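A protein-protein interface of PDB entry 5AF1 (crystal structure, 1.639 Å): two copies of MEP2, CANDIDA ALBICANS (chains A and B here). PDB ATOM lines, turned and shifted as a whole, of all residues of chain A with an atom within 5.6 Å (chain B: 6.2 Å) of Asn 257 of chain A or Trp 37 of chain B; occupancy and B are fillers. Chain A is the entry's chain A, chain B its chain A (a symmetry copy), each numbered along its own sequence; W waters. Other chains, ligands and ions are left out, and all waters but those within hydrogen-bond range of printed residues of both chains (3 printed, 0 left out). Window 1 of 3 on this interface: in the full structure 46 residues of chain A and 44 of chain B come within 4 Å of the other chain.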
ATOM      1  N   THR A 227     -31.277   9.435  11.081  1.00  0.00           N
ATOM      2  CA  THR A 227     -31.286   8.758   9.785  1.00  0.00           C
ATOM      3  C   THR A 227     -30.172   7.708   9.736  1.00  0.00           C
ATOM      4  O   THR A 227     -30.366   6.602   9.211  1.00  0.00           O
ATOM      5  CB  THR A 227     -31.135   9.774   8.636  1.00  0.00           C
ATOM      6  OG1 THR A 227     -32.201  10.731   8.725  1.00  0.00           O
ATOM      7  CG2 THR A 227     -31.223   9.089   7.276  1.00  0.00           C
ATOM      8  N   ILE A 228     -29.020   8.047  10.308  1.00  0.00           N
ATOM      9  CA  ILE A 228     -27.915   7.088  10.434  1.00  0.00           C
ATOM     10  C   ILE A 228     -28.331   5.848  11.214  1.00  0.00           C
ATOM     11  O   ILE A 228     -28.138   4.711  10.739  1.00  0.00           O
ATOM     12  CB  ILE A 228     -26.695   7.735  11.132  1.00  0.00           C
ATOM     13  CG1 ILE A 228     -26.029   8.743  10.197  1.00  0.00           C
ATOM     14  CG2 ILE A 228     -25.682   6.655  11.537  1.00  0.00           C
ATOM     15  CD1 ILE A 228     -25.139   9.746  10.936  1.00  0.00           C
ATOM     16  N   TRP A 231     -31.055   3.852   9.092  1.00  0.00           N
ATOM     17  CA  TRP A 231     -30.530   3.121   7.923  1.00  0.00           C
ATOM     18  C   TRP A 231     -29.664   1.922   8.366  1.00  0.00           C
ATOM     19  O   TRP A 231     -29.816   0.794   7.873  1.00  0.00           O
ATOM     20  CB  TRP A 231     -29.748   4.123   7.057  1.00  0.00           C
ATOM     21  CG  TRP A 231     -29.318   3.705   5.690  1.00  0.00           C
ATOM     22  CD1 TRP A 231     -29.002   2.439   5.245  1.00  0.00           C
ATOM     23  CD2 TRP A 231     -29.115   4.583   4.589  1.00  0.00           C
ATOM     24  NE1 TRP A 231     -28.614   2.499   3.917  1.00  0.00           N
ATOM     25  CE2 TRP A 231     -28.670   3.807   3.503  1.00  0.00           C
ATOM     26  CE3 TRP A 231     -29.257   5.971   4.422  1.00  0.00           C
ATOM     27  CZ2 TRP A 231     -28.382   4.368   2.259  1.00  0.00           C
ATOM     28  CZ3 TRP A 231     -28.961   6.526   3.197  1.00  0.00           C
ATOM     29  CH2 TRP A 231     -28.533   5.727   2.124  1.00  0.00           C
ATOM     30  N   PHE A 232     -28.766   2.165   9.315  1.00  0.00           N
ATOM     31  CA  PHE A 232     -27.933   1.105   9.920  1.00  0.00           C
ATOM     32  C   PHE A 232     -28.792  -0.035  10.476  1.00  0.00           C
ATOM     33  O   PHE A 232     -28.576  -1.231  10.153  1.00  0.00           O
ATOM     34  CB  PHE A 232     -27.072   1.764  11.010  1.00  0.00           C
ATOM     35  CG  PHE A 232     -26.241   0.826  11.848  1.00  0.00           C
ATOM     36  CD1 PHE A 232     -25.054   0.289  11.354  1.00  0.00           C
ATOM     37  CD2 PHE A 232     -26.586   0.584  13.181  1.00  0.00           C
ATOM     38  CE1 PHE A 232     -24.251  -0.507  12.160  1.00  0.00           C
ATOM     39  CE2 PHE A 232     -25.795  -0.222  13.999  1.00  0.00           C
ATOM     40  CZ  PHE A 232     -24.628  -0.773  13.486  1.00  0.00           C
ATOM     41  N   TYR A 235     -30.955  -2.638   8.145  1.00  0.00           N
ATOM     42  CA  TYR A 235     -30.405  -3.901   7.650  1.00  0.00           C
ATOM     43  C   TYR A 235     -30.879  -5.085   8.493  1.00  0.00           C
ATOM     44  O   TYR A 235     -31.089  -6.179   7.954  1.00  0.00           O
ATOM     45  CB  TYR A 235     -28.881  -3.850   7.630  1.00  0.00           C
ATOM     46  CG  TYR A 235     -28.335  -2.869   6.630  1.00  0.00           C
ATOM     47  CD1 TYR A 235     -28.515  -3.055   5.269  1.00  0.00           C
ATOM     48  CD2 TYR A 235     -27.638  -1.733   7.059  1.00  0.00           C
ATOM     49  CE1 TYR A 235     -28.012  -2.147   4.342  1.00  0.00           C
ATOM     50  CE2 TYR A 235     -27.131  -0.824   6.149  1.00  0.00           C
ATOM     51  CZ  TYR A 235     -27.325  -1.025   4.794  1.00  0.00           C
ATOM     52  OH  TYR A 235     -26.825  -0.124   3.873  1.00  0.00           O
ATOM     53  N   ALA A 252     -32.070  -8.891   0.303  1.00  0.00           N
ATOM     54  CA  ALA A 252     -32.946  -7.891   0.930  1.00  0.00           C
ATOM     55  C   ALA A 252     -32.157  -6.667   1.409  1.00  0.00           C
ATOM     56  O   ALA A 252     -32.640  -5.537   1.316  1.00  0.00           O
ATOM     57  CB  ALA A 252     -33.719  -8.516   2.097  1.00  0.00           C
ATOM     58  N   CYS A 253     -30.948  -6.886   1.924  1.00  0.00           N
ATOM     59  CA  CYS A 253     -30.097  -5.763   2.349  1.00  0.00           C
ATOM     60  C   CYS A 253     -29.648  -4.887   1.180  1.00  0.00           C
ATOM     61  O   CYS A 253     -29.563  -3.657   1.304  1.00  0.00           O
ATOM     62  CB  CYS A 253     -28.867  -6.278   3.100  1.00  0.00           C
ATOM     63  SG  CYS A 253     -29.216  -6.918   4.776  1.00  0.00           S
ATOM     64  N   VAL A 254     -29.337  -5.516   0.050  1.00  0.00           N
ATOM     65  CA  VAL A 254     -28.948  -4.761  -1.137  1.00  0.00           C
ATOM     66  C   VAL A 254     -30.121  -3.891  -1.596  1.00  0.00           C
ATOM     67  O   VAL A 254     -29.938  -2.707  -1.900  1.00  0.00           O
ATOM     68  CB  VAL A 254     -28.480  -5.704  -2.274  1.00  0.00           C
ATOM     69  CG1 VAL A 254     -28.373  -4.958  -3.597  1.00  0.00           C
ATOM     70  CG2 VAL A 254     -27.142  -6.348  -1.897  1.00  0.00           C
ATOM     71  N   ASN A 255     -31.327  -4.466  -1.600  1.00  0.00           N
ATOM     72  CA  ASN A 255     -32.539  -3.715  -1.944  1.00  0.00           C
ATOM     73  C   ASN A 255     -32.785  -2.558  -0.977  1.00  0.00           C
ATOM     74  O   ASN A 255     -33.193  -1.470  -1.390  1.00  0.00           O
ATOM     75  CB  ASN A 255     -33.767  -4.641  -1.966  1.00  0.00           C
ATOM     76  CG  ASN A 255     -33.875  -5.422  -3.254  1.00  0.00           C
ATOM     77  OD1 ASN A 255     -33.213  -5.100  -4.243  1.00  0.00           O
ATOM     78  ND2 ASN A 255     -34.707  -6.461  -3.252  1.00  0.00           N
ATOM     79  N   THR A 256     -32.551  -2.811   0.304  1.00  0.00           N
ATOM     80  CA  THR A 256     -32.758  -1.816   1.362  1.00  0.00           C
ATOM     81  C   THR A 256     -31.861  -0.594   1.151  1.00  0.00           C
ATOM     82  O   THR A 256     -32.326   0.547   1.163  1.00  0.00           O
ATOM     83  CB  THR A 256     -32.497  -2.444   2.750  1.00  0.00           C
ATOM     84  OG1 THR A 256     -33.443  -3.505   2.975  1.00  0.00           O
ATOM     85  CG2 THR A 256     -32.660  -1.415   3.874  1.00  0.00           C
ATOM     86  N   ASN A 257     -30.576  -0.855   0.943  1.00  0.00           N
ATOM     87  CA  ASN A 257     -29.577   0.185   0.715  1.00  0.00           C
ATOM     88  C   ASN A 257     -29.898   0.998  -0.553  1.00  0.00           C
ATOM     89  O   ASN A 257     -29.852   2.229  -0.549  1.00  0.00           O
ATOM     90  CB  ASN A 257     -28.197  -0.485   0.640  1.00  0.00           C
ATOM     91  CG  ASN A 257     -27.048   0.505   0.560  1.00  0.00           C
ATOM     92  OD1 ASN A 257     -27.033   1.534   1.242  1.00  0.00           O
ATOM     93  ND2 ASN A 257     -26.072   0.190  -0.283  1.00  0.00           N
ATOM     94  N   LEU A 258     -30.278   0.307  -1.628  1.00  0.00           N
ATOM     95  CA  LEU A 258     -30.538   0.984  -2.894  1.00  0.00           C
ATOM     96  C   LEU A 258     -31.820   1.815  -2.826  1.00  0.00           C
ATOM     97  O   LEU A 258     -31.888   2.911  -3.387  1.00  0.00           O
ATOM     98  CB  LEU A 258     -30.604  -0.041  -4.040  1.00  0.00           C
ATOM     99  CG  LEU A 258     -30.657   0.538  -5.454  1.00  0.00           C
ATOM    100  CD1 LEU A 258     -29.528   1.525  -5.703  1.00  0.00           C
ATOM    101  CD2 LEU A 258     -30.582  -0.613  -6.465  1.00  0.00           C
ATOM    102  N   ALA A 259     -32.839   1.314  -2.130  1.00  0.00           N
ATOM    103  CA  ALA A 259     -34.080   2.082  -1.992  1.00  0.00           C
ATOM    104  C   ALA A 259     -33.848   3.342  -1.151  1.00  0.00           C
ATOM    105  O   ALA A 259     -34.373   4.414  -1.463  1.00  0.00           O
ATOM    106  CB  ALA A 259     -35.183   1.228  -1.368  1.00  0.00           C
ATOM    107  N   ALA A 260     -33.076   3.213  -0.079  1.00  0.00           N
ATOM    108  CA  ALA A 260     -32.741   4.382   0.738  1.00  0.00           C
ATOM    109  C   ALA A 260     -32.001   5.408  -0.098  1.00  0.00           C
ATOM    110  O   ALA A 260     -32.311   6.597  -0.072  1.00  0.00           O
ATOM    111  CB  ALA A 260     -31.883   3.965   1.943  1.00  0.00           C
ATOM    112  N   ALA A 261     -31.027   4.928  -0.863  1.00  0.00           N
ATOM    113  CA  ALA A 261     -30.149   5.798  -1.633  1.00  0.00           C
ATOM    114  C   ALA A 261     -30.922   6.575  -2.692  1.00  0.00           C
ATOM    115  O   ALA A 261     -30.740   7.793  -2.846  1.00  0.00           O
ATOM    116  CB  ALA A 261     -29.034   4.968  -2.288  1.00  0.00           C
ATOM    117  N   THR A 262     -31.785   5.872  -3.424  1.00  0.00           N
ATOM    118  CA  THR A 262     -32.527   6.513  -4.498  1.00  0.00           C
ATOM    119  C   THR A 262     -33.657   7.368  -3.942  1.00  0.00           C
ATOM    120  O   THR A 262     -34.001   8.388  -4.532  1.00  0.00           O
ATOM    121  CB  THR A 262     -33.061   5.474  -5.509  1.00  0.00           C
ATOM    122  OG1 THR A 262     -33.884   4.519  -4.842  1.00  0.00           O
ATOM    123  CG2 THR A 262     -31.891   4.757  -6.149  1.00  0.00           C
ATOM    124  N   LEU A 292     -36.665   3.676   2.570  1.00  0.00           N
ATOM    125  CA  LEU A 292     -36.598   2.576   3.537  1.00  0.00           C
ATOM    126  C   LEU A 292     -37.999   2.059   3.889  1.00  0.00           C
ATOM    127  O   LEU A 292     -38.239   0.849   3.927  1.00  0.00           O
ATOM    128  CB  LEU A 292     -35.842   3.026   4.798  1.00  0.00           C
ATOM    129  CG  LEU A 292     -34.337   3.217   4.568  1.00  0.00           C
ATOM    130  CD1 LEU A 292     -33.676   4.015   5.700  1.00  0.00           C
ATOM    131  CD2 LEU A 292     -33.634   1.874   4.418  1.00  0.00           C
ATOM    132  N   ALA B  32     -20.599  -7.817   8.912  1.00  0.00           N
ATOM    133  CA  ALA B  32     -19.467  -6.936   8.620  1.00  0.00           C
ATOM    134  C   ALA B  32     -19.871  -5.826   7.651  1.00  0.00           C
ATOM    135  O   ALA B  32     -19.369  -4.705   7.750  1.00  0.00           O
ATOM    136  CB  ALA B  32     -18.293  -7.757   8.046  1.00  0.00           C
ATOM    137  N   SER B  33     -20.768  -6.143   6.714  1.00  0.00           N
ATOM    138  CA  SER B  33     -21.291  -5.138   5.777  1.00  0.00           C
ATOM    139  C   SER B  33     -21.995  -4.007   6.517  1.00  0.00           C
ATOM    140  O   SER B  33     -21.820  -2.830   6.192  1.00  0.00           O
ATOM    141  CB  SER B  33     -22.266  -5.781   4.780  1.00  0.00           C
ATOM    142  OG  SER B  33     -21.601  -6.773   4.006  1.00  0.00           O
ATOM    143  N   VAL B  34     -22.819  -4.382   7.489  1.00  0.00           N
ATOM    144  CA  VAL B  34     -23.587  -3.417   8.249  1.00  0.00           C
ATOM    145  C   VAL B  34     -22.619  -2.540   9.051  1.00  0.00           C
ATOM    146  O   VAL B  34     -22.802  -1.314   9.144  1.00  0.00           O
ATOM    147  CB  VAL B  34     -24.600  -4.136   9.172  1.00  0.00           C
ATOM    148  CG1 VAL B  34     -25.333  -3.141  10.056  1.00  0.00           C
ATOM    149  CG2 VAL B  34     -25.612  -4.937   8.322  1.00  0.00           C
ATOM    150  N   LEU B  35     -21.588  -3.164   9.615  1.00  0.00           N
ATOM    151  CA  LEU B  35     -20.569  -2.422  10.368  1.00  0.00           C
ATOM    152  C   LEU B  35     -19.798  -1.443   9.488  1.00  0.00           C
ATOM    153  O   LEU B  35     -19.543  -0.308   9.910  1.00  0.00           O
ATOM    154  CB  LEU B  35     -19.595  -3.399  11.050  1.00  0.00           C
ATOM    155  CG  LEU B  35     -20.214  -4.235  12.186  1.00  0.00           C
ATOM    156  CD1 LEU B  35     -19.211  -5.292  12.665  1.00  0.00           C
ATOM    157  CD2 LEU B  35     -20.643  -3.340  13.349  1.00  0.00           C
ATOM    158  N   VAL B  36     -19.444  -1.842   8.269  1.00  0.00           N
ATOM    159  CA  VAL B  36     -18.727  -0.902   7.403  1.00  0.00           C
ATOM    160  C   VAL B  36     -19.647   0.263   7.041  1.00  0.00           C
ATOM    161  O   VAL B  36     -19.167   1.401   6.943  1.00  0.00           O
ATOM    162  CB  VAL B  36     -18.169  -1.572   6.130  1.00  0.00           C
ATOM    163  CG1 VAL B  36     -17.457  -0.534   5.228  1.00  0.00           C
ATOM    164  CG2 VAL B  36     -17.161  -2.656   6.512  1.00  0.00           C
ATOM    165  N   TRP B  37     -20.951   0.020   6.903  1.00  0.00           N
ATOM    166  CA  TRP B  37     -21.858   1.117   6.518  1.00  0.00           C
ATOM    167  C   TRP B  37     -21.742   2.276   7.516  1.00  0.00           C
ATOM    168  O   TRP B  37     -21.689   3.453   7.110  1.00  0.00           O
ATOM    169  CB  TRP B  37     -23.335   0.656   6.393  1.00  0.00           C
ATOM    170  CG  TRP B  37     -24.146   1.735   5.751  1.00  0.00           C
ATOM    171  CD1 TRP B  37     -24.312   1.969   4.405  1.00  0.00           C
ATOM    172  CD2 TRP B  37     -24.800   2.816   6.428  1.00  0.00           C
ATOM    173  NE1 TRP B  37     -25.063   3.119   4.213  1.00  0.00           N
ATOM    174  CE2 TRP B  37     -25.380   3.646   5.439  1.00  0.00           C
ATOM    175  CE3 TRP B  37     -24.984   3.135   7.773  1.00  0.00           C
ATOM    176  CZ2 TRP B  37     -26.107   4.797   5.759  1.00  0.00           C
ATOM    177  CZ3 TRP B  37     -25.717   4.280   8.093  1.00  0.00           C
ATOM    178  CH2 TRP B  37     -26.270   5.089   7.087  1.00  0.00           C
ATOM    179  N   ILE B  38     -21.656   1.978   8.813  1.00  0.00           N
ATOM    180  CA  ILE B  38     -21.656   3.091   9.777  1.00  0.00           C
ATOM    181  C   ILE B  38     -20.322   3.845   9.795  1.00  0.00           C
ATOM    182  O   ILE B  38     -20.244   4.957  10.350  1.00  0.00           O
ATOM    183  CB  ILE B  38     -22.056   2.603  11.203  1.00  0.00           C
ATOM    184  CG1 ILE B  38     -22.686   3.752  12.012  1.00  0.00           C
ATOM    185  CG2 ILE B  38     -20.875   1.973  11.947  1.00  0.00           C
ATOM    186  CD1 ILE B  38     -23.311   3.293  13.317  1.00  0.00           C
ATOM    187  N   MET B  39     -19.297   3.309   9.134  1.00  0.00           N
ATOM    188  CA  MET B  39     -18.053   4.065   8.933  1.00  0.00           C
ATOM    189  C   MET B  39     -18.267   5.275   8.034  1.00  0.00           C
ATOM    190  O   MET B  39     -17.496   6.241   8.099  1.00  0.00           O
ATOM    191  CB  MET B  39     -16.964   3.174   8.340  1.00  0.00           C
ATOM    192  CG  MET B  39     -16.588   2.043   9.282  1.00  0.00           C
ATOM    193  SD  MET B  39     -15.348   0.962   8.534  1.00  0.00           S
ATOM    194  CE  MET B  39     -13.925   2.052   8.395  1.00  0.00           C
ATOM    195  N   ILE B  40     -19.311   5.232   7.214  1.00  0.00           N
ATOM    196  CA  ILE B  40     -19.549   6.321   6.266  1.00  0.00           C
ATOM    197  C   ILE B  40     -19.856   7.619   7.042  1.00  0.00           C
ATOM    198  O   ILE B  40     -19.143   8.625   6.861  1.00  0.00           O
ATOM    199  CB  ILE B  40     -20.686   5.959   5.262  1.00  0.00           C
ATOM    200  CG1 ILE B  40     -20.323   4.704   4.458  1.00  0.00           C
ATOM    201  CG2 ILE B  40     -20.984   7.152   4.331  1.00  0.00           C
ATOM    202  CD1 ILE B  40     -21.581   4.056   3.844  1.00  0.00           C
ATOM    203  N   PRO B  41     -20.871   7.613   7.931  1.00  0.00           N
ATOM    204  CA  PRO B  41     -21.020   8.834   8.749  1.00  0.00           C
ATOM    205  C   PRO B  41     -19.867   9.041   9.728  1.00  0.00           C
ATOM    206  O   PRO B  41     -19.612  10.193  10.134  1.00  0.00           O
ATOM    207  CB  PRO B  41     -22.336   8.602   9.491  1.00  0.00           C
ATOM    208  CG  PRO B  41     -22.503   7.071   9.503  1.00  0.00           C
ATOM    209  CD  PRO B  41     -21.990   6.669   8.158  1.00  0.00           C
ATOM    210  N   GLY B  42     -19.163   7.968  10.084  1.00  0.00           N
ATOM    211  CA  GLY B  42     -17.962   8.099  10.895  1.00  0.00           C
ATOM    212  C   GLY B  42     -16.963   9.048  10.237  1.00  0.00           C
ATOM    213  O   GLY B  42     -16.462   9.954  10.895  1.00  0.00           O
ATOM    214  N   LEU B  64     -24.314  11.166   4.378  1.00  0.00           N
ATOM    215  CA  LEU B  64     -25.530  10.515   3.883  1.00  0.00           C
ATOM    216  C   LEU B  64     -25.661  10.738   2.385  1.00  0.00           C
ATOM    217  O   LEU B  64     -26.056   9.840   1.652  1.00  0.00           O
ATOM    218  CB  LEU B  64     -26.775  11.025   4.610  1.00  0.00           C
ATOM    219  CG  LEU B  64     -26.851  10.634   6.090  1.00  0.00           C
ATOM    220  CD1 LEU B  64     -28.102  11.221   6.723  1.00  0.00           C
ATOM    221  CD2 LEU B  64     -26.809   9.114   6.243  1.00  0.00           C
ATOM    222  N   ALA B  67     -23.375   8.294   0.857  1.00  0.00           N
ATOM    223  CA  ALA B  67     -23.956   6.934   0.931  1.00  0.00           C
ATOM    224  C   ALA B  67     -24.955   6.710  -0.206  1.00  0.00           C
ATOM    225  O   ALA B  67     -25.044   5.603  -0.765  1.00  0.00           O
ATOM    226  CB  ALA B  67     -24.625   6.722   2.272  1.00  0.00           C
ATOM    227  N   ALA B  71     -24.017   4.246  -3.403  1.00  0.00           N
ATOM    228  CA  ALA B  71     -24.863   3.050  -3.568  1.00  0.00           C
ATOM    229  C   ALA B  71     -25.425   2.995  -4.974  1.00  0.00           C
ATOM    230  O   ALA B  71     -25.494   1.917  -5.589  1.00  0.00           O
ATOM    231  CB  ALA B  71     -25.986   3.032  -2.563  1.00  0.00           C
ATOM    232  N   LEU B 119     -22.871  -6.552  -1.606  1.00  0.00           N
ATOM    233  CA  LEU B 119     -23.265  -5.777  -0.422  1.00  0.00           C
ATOM    234  C   LEU B 119     -22.043  -5.291   0.354  1.00  0.00           C
ATOM    235  O   LEU B 119     -21.911  -4.090   0.649  1.00  0.00           O
ATOM    236  CB  LEU B 119     -24.166  -6.627   0.485  1.00  0.00           C
ATOM    237  CG  LEU B 119     -24.598  -5.936   1.782  1.00  0.00           C
ATOM    238  CD1 LEU B 119     -25.586  -4.825   1.451  1.00  0.00           C
ATOM    239  CD2 LEU B 119     -25.216  -6.959   2.728  1.00  0.00           C
ATOM    240  N   GLY B 122     -19.624  -2.941  -1.728  1.00  0.00           N
ATOM    241  CA  GLY B 122     -20.267  -1.663  -1.990  1.00  0.00           C
ATOM    242  C   GLY B 122     -20.017  -0.683  -0.848  1.00  0.00           C
ATOM    243  O   GLY B 122     -19.916   0.532  -1.063  1.00  0.00           O
ATOM    244  N   MET B 123     -19.915  -1.204   0.373  1.00  0.00           N
ATOM    245  CA  MET B 123     -19.679  -0.352   1.540  1.00  0.00           C
ATOM    246  C   MET B 123     -18.303   0.314   1.487  1.00  0.00           C
ATOM    247  O   MET B 123     -18.142   1.457   1.931  1.00  0.00           O
ATOM    248  CB  MET B 123     -19.811  -1.150   2.839  1.00  0.00           C
ATOM    249  CG  MET B 123     -21.140  -1.894   3.012  1.00  0.00           C
ATOM    250  SD  MET B 123     -22.565  -0.792   2.820  1.00  0.00           S
ATOM    251  CE  MET B 123     -23.920  -1.922   3.226  1.00  0.00           C
ATOM    252  N   ALA B 126     -18.450   3.270  -0.736  1.00  0.00           N
ATOM    253  CA  ALA B 126     -19.130   4.387  -0.071  1.00  0.00           C
ATOM    254  C   ALA B 126     -18.231   5.078   0.951  1.00  0.00           C
ATOM    255  O   ALA B 126     -18.241   6.306   1.067  1.00  0.00           O
ATOM    256  CB  ALA B 126     -20.407   3.905   0.594  1.00  0.00           C
ATOM    257  N   VAL B 127     -17.460   4.300   1.703  1.00  0.00           N
ATOM    258  CA  VAL B 127     -16.503   4.905   2.639  1.00  0.00           C
ATOM    259  C   VAL B 127     -15.512   5.781   1.860  1.00  0.00           C
ATOM    260  O   VAL B 127     -15.179   6.899   2.270  1.00  0.00           O
ATOM    261  CB  VAL B 127     -15.752   3.825   3.449  1.00  0.00           C
ATOM    262  CG1 VAL B 127     -14.553   4.427   4.208  1.00  0.00           C
ATOM    263  CG2 VAL B 127     -16.716   3.122   4.419  1.00  0.00           C
HETATM  264  O   HOH W   1     -25.045   3.384   1.214  1.00  0.00           O
HETATM  265  O   HOH W   2     -23.364   1.430   0.081  1.00  0.00           O
HETATM  266  O   HOH W   3     -23.393  -1.963  -0.397  1.00  0.00           O
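OH of Tyr 235 of chain A sits at hydrogen-bond distance from OD1 of Asn 257 of chain A, at 3.1 Å.
The indole nitrogen of Trp 231 of chain A lies within hydrogen-bond range of the side-chain hydroxyl of Tyr 235 of chain A (3.2 Å).
The indole nitrogen (NE1) of Trp 231 of chain A sits at hydrogen-bond distance from the side-chain amide oxygen (OD1) of Asn 257 of chain A (3.3 Å).
O of Tyr 235 of chain A lies within hydrogen-bond range of SG of Cys 253 of chain A (3.8 Å).
No position is printed for both chains.
Thr 227 of chain A touches Leu 64 of chain B (CG2 to CD1, 3.8 Å).
O of Ile 228 of chain A touches CZ3 of Trp 37 of chain B, at 3.6 Å.
CB of Pro 41 of chain B touches CD1 of Ile 228 of chain A, at 3.4 Å.
Trp 231 of chain A touches Trp 37 of chain B.
CZ3 of Trp 37 of chain B touches N of Phe 232 of chain A (3.9 Å).
Phe 232 of chain A touches Ile 38 of chain B (CD1 to CB, 3.8 Å).
Tyr 235 of chain A touches Trp 37 of chain B.
Val 254 of chain A touches Leu 119 of chain B (CG2 to CB, 3.8 Å).
Asn 257 of chain A touches Ala 71 of chain B (ND2 to CB, 3.6 Å).
CB of Ala 71 of chain B touches CB of Ala 261 of chain A, at 3.6 Å.
Water W1 lies within hydrogen-bond range of OD1 of Asn 257 of chain A (2.7 Å), O of Ala 67 of chain B (3.0 Å) and NE1 of Trp 37 of chain B (3.0 Å).
Water W3 lies within hydrogen-bond range of the backbone carbonyl oxygen of Leu 119 of chain B (2.8 Å), the side-chain amide nitrogen of Asn 257 of chain A (3.4 Å) and the side-chain sulfur of Met 123 of chain B (3.5 Å).
Water W2 bridges ND2 of Asn 257 of chain A (3.0 Å) and SD of Met 123 of chain B (3.6 Å).
Printed residues of chain B within 4 Å of Trp 231 of chain A: Trp 37 (3.2 Å).
Printed residues of chain B within 4 Å of Phe 232 of chain A: Val 34 (3.4 Å), Trp 37 (3.9 Å) and Ile 38 (3.8 Å).
Trp 37 of chain B touches just these residues of chain A: Ile 228, Trp 231, Phe 232, Tyr 235 and Asn 257.
Printed residues of chain A within 4 Å of Ala 71 of chain B: Asn 257 and Ala 261.
Printed residues of chain A within 4 Å of Leu 119 of chain B: Cys 253 (3.7 Å) and Val 254 (3.8 Å).
The nearest residue of chain A that does not touch Trp 37 of chain B is Thr 227 of chain A (4.9 Å).
Of the 17 printed residues of chain A, 9 touch a printed residue of chain B.
Hydrophobic or aromatic side chains of chain A that line the printed part of chain B: Ile 228, Trp 231, Phe 232, Tyr 235, Val 254 and Ala 261.
Of the 19 printed residues of chain B, 8 touch a printed residue of chain A.
Printed residues of chain B that touch a printed residue of chain A: Val 34, Trp 37, Ile 38, Pro 41, Leu 64, Ala 71, Leu 119 and Met 123.
Hydrophobic or aromatic side chains of chain B within 4 Å of the printed part of chain A: Val 34, Trp 37, Ile 38, Pro 41, Leu 64, Ala 71, Leu 119 and Met 123.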
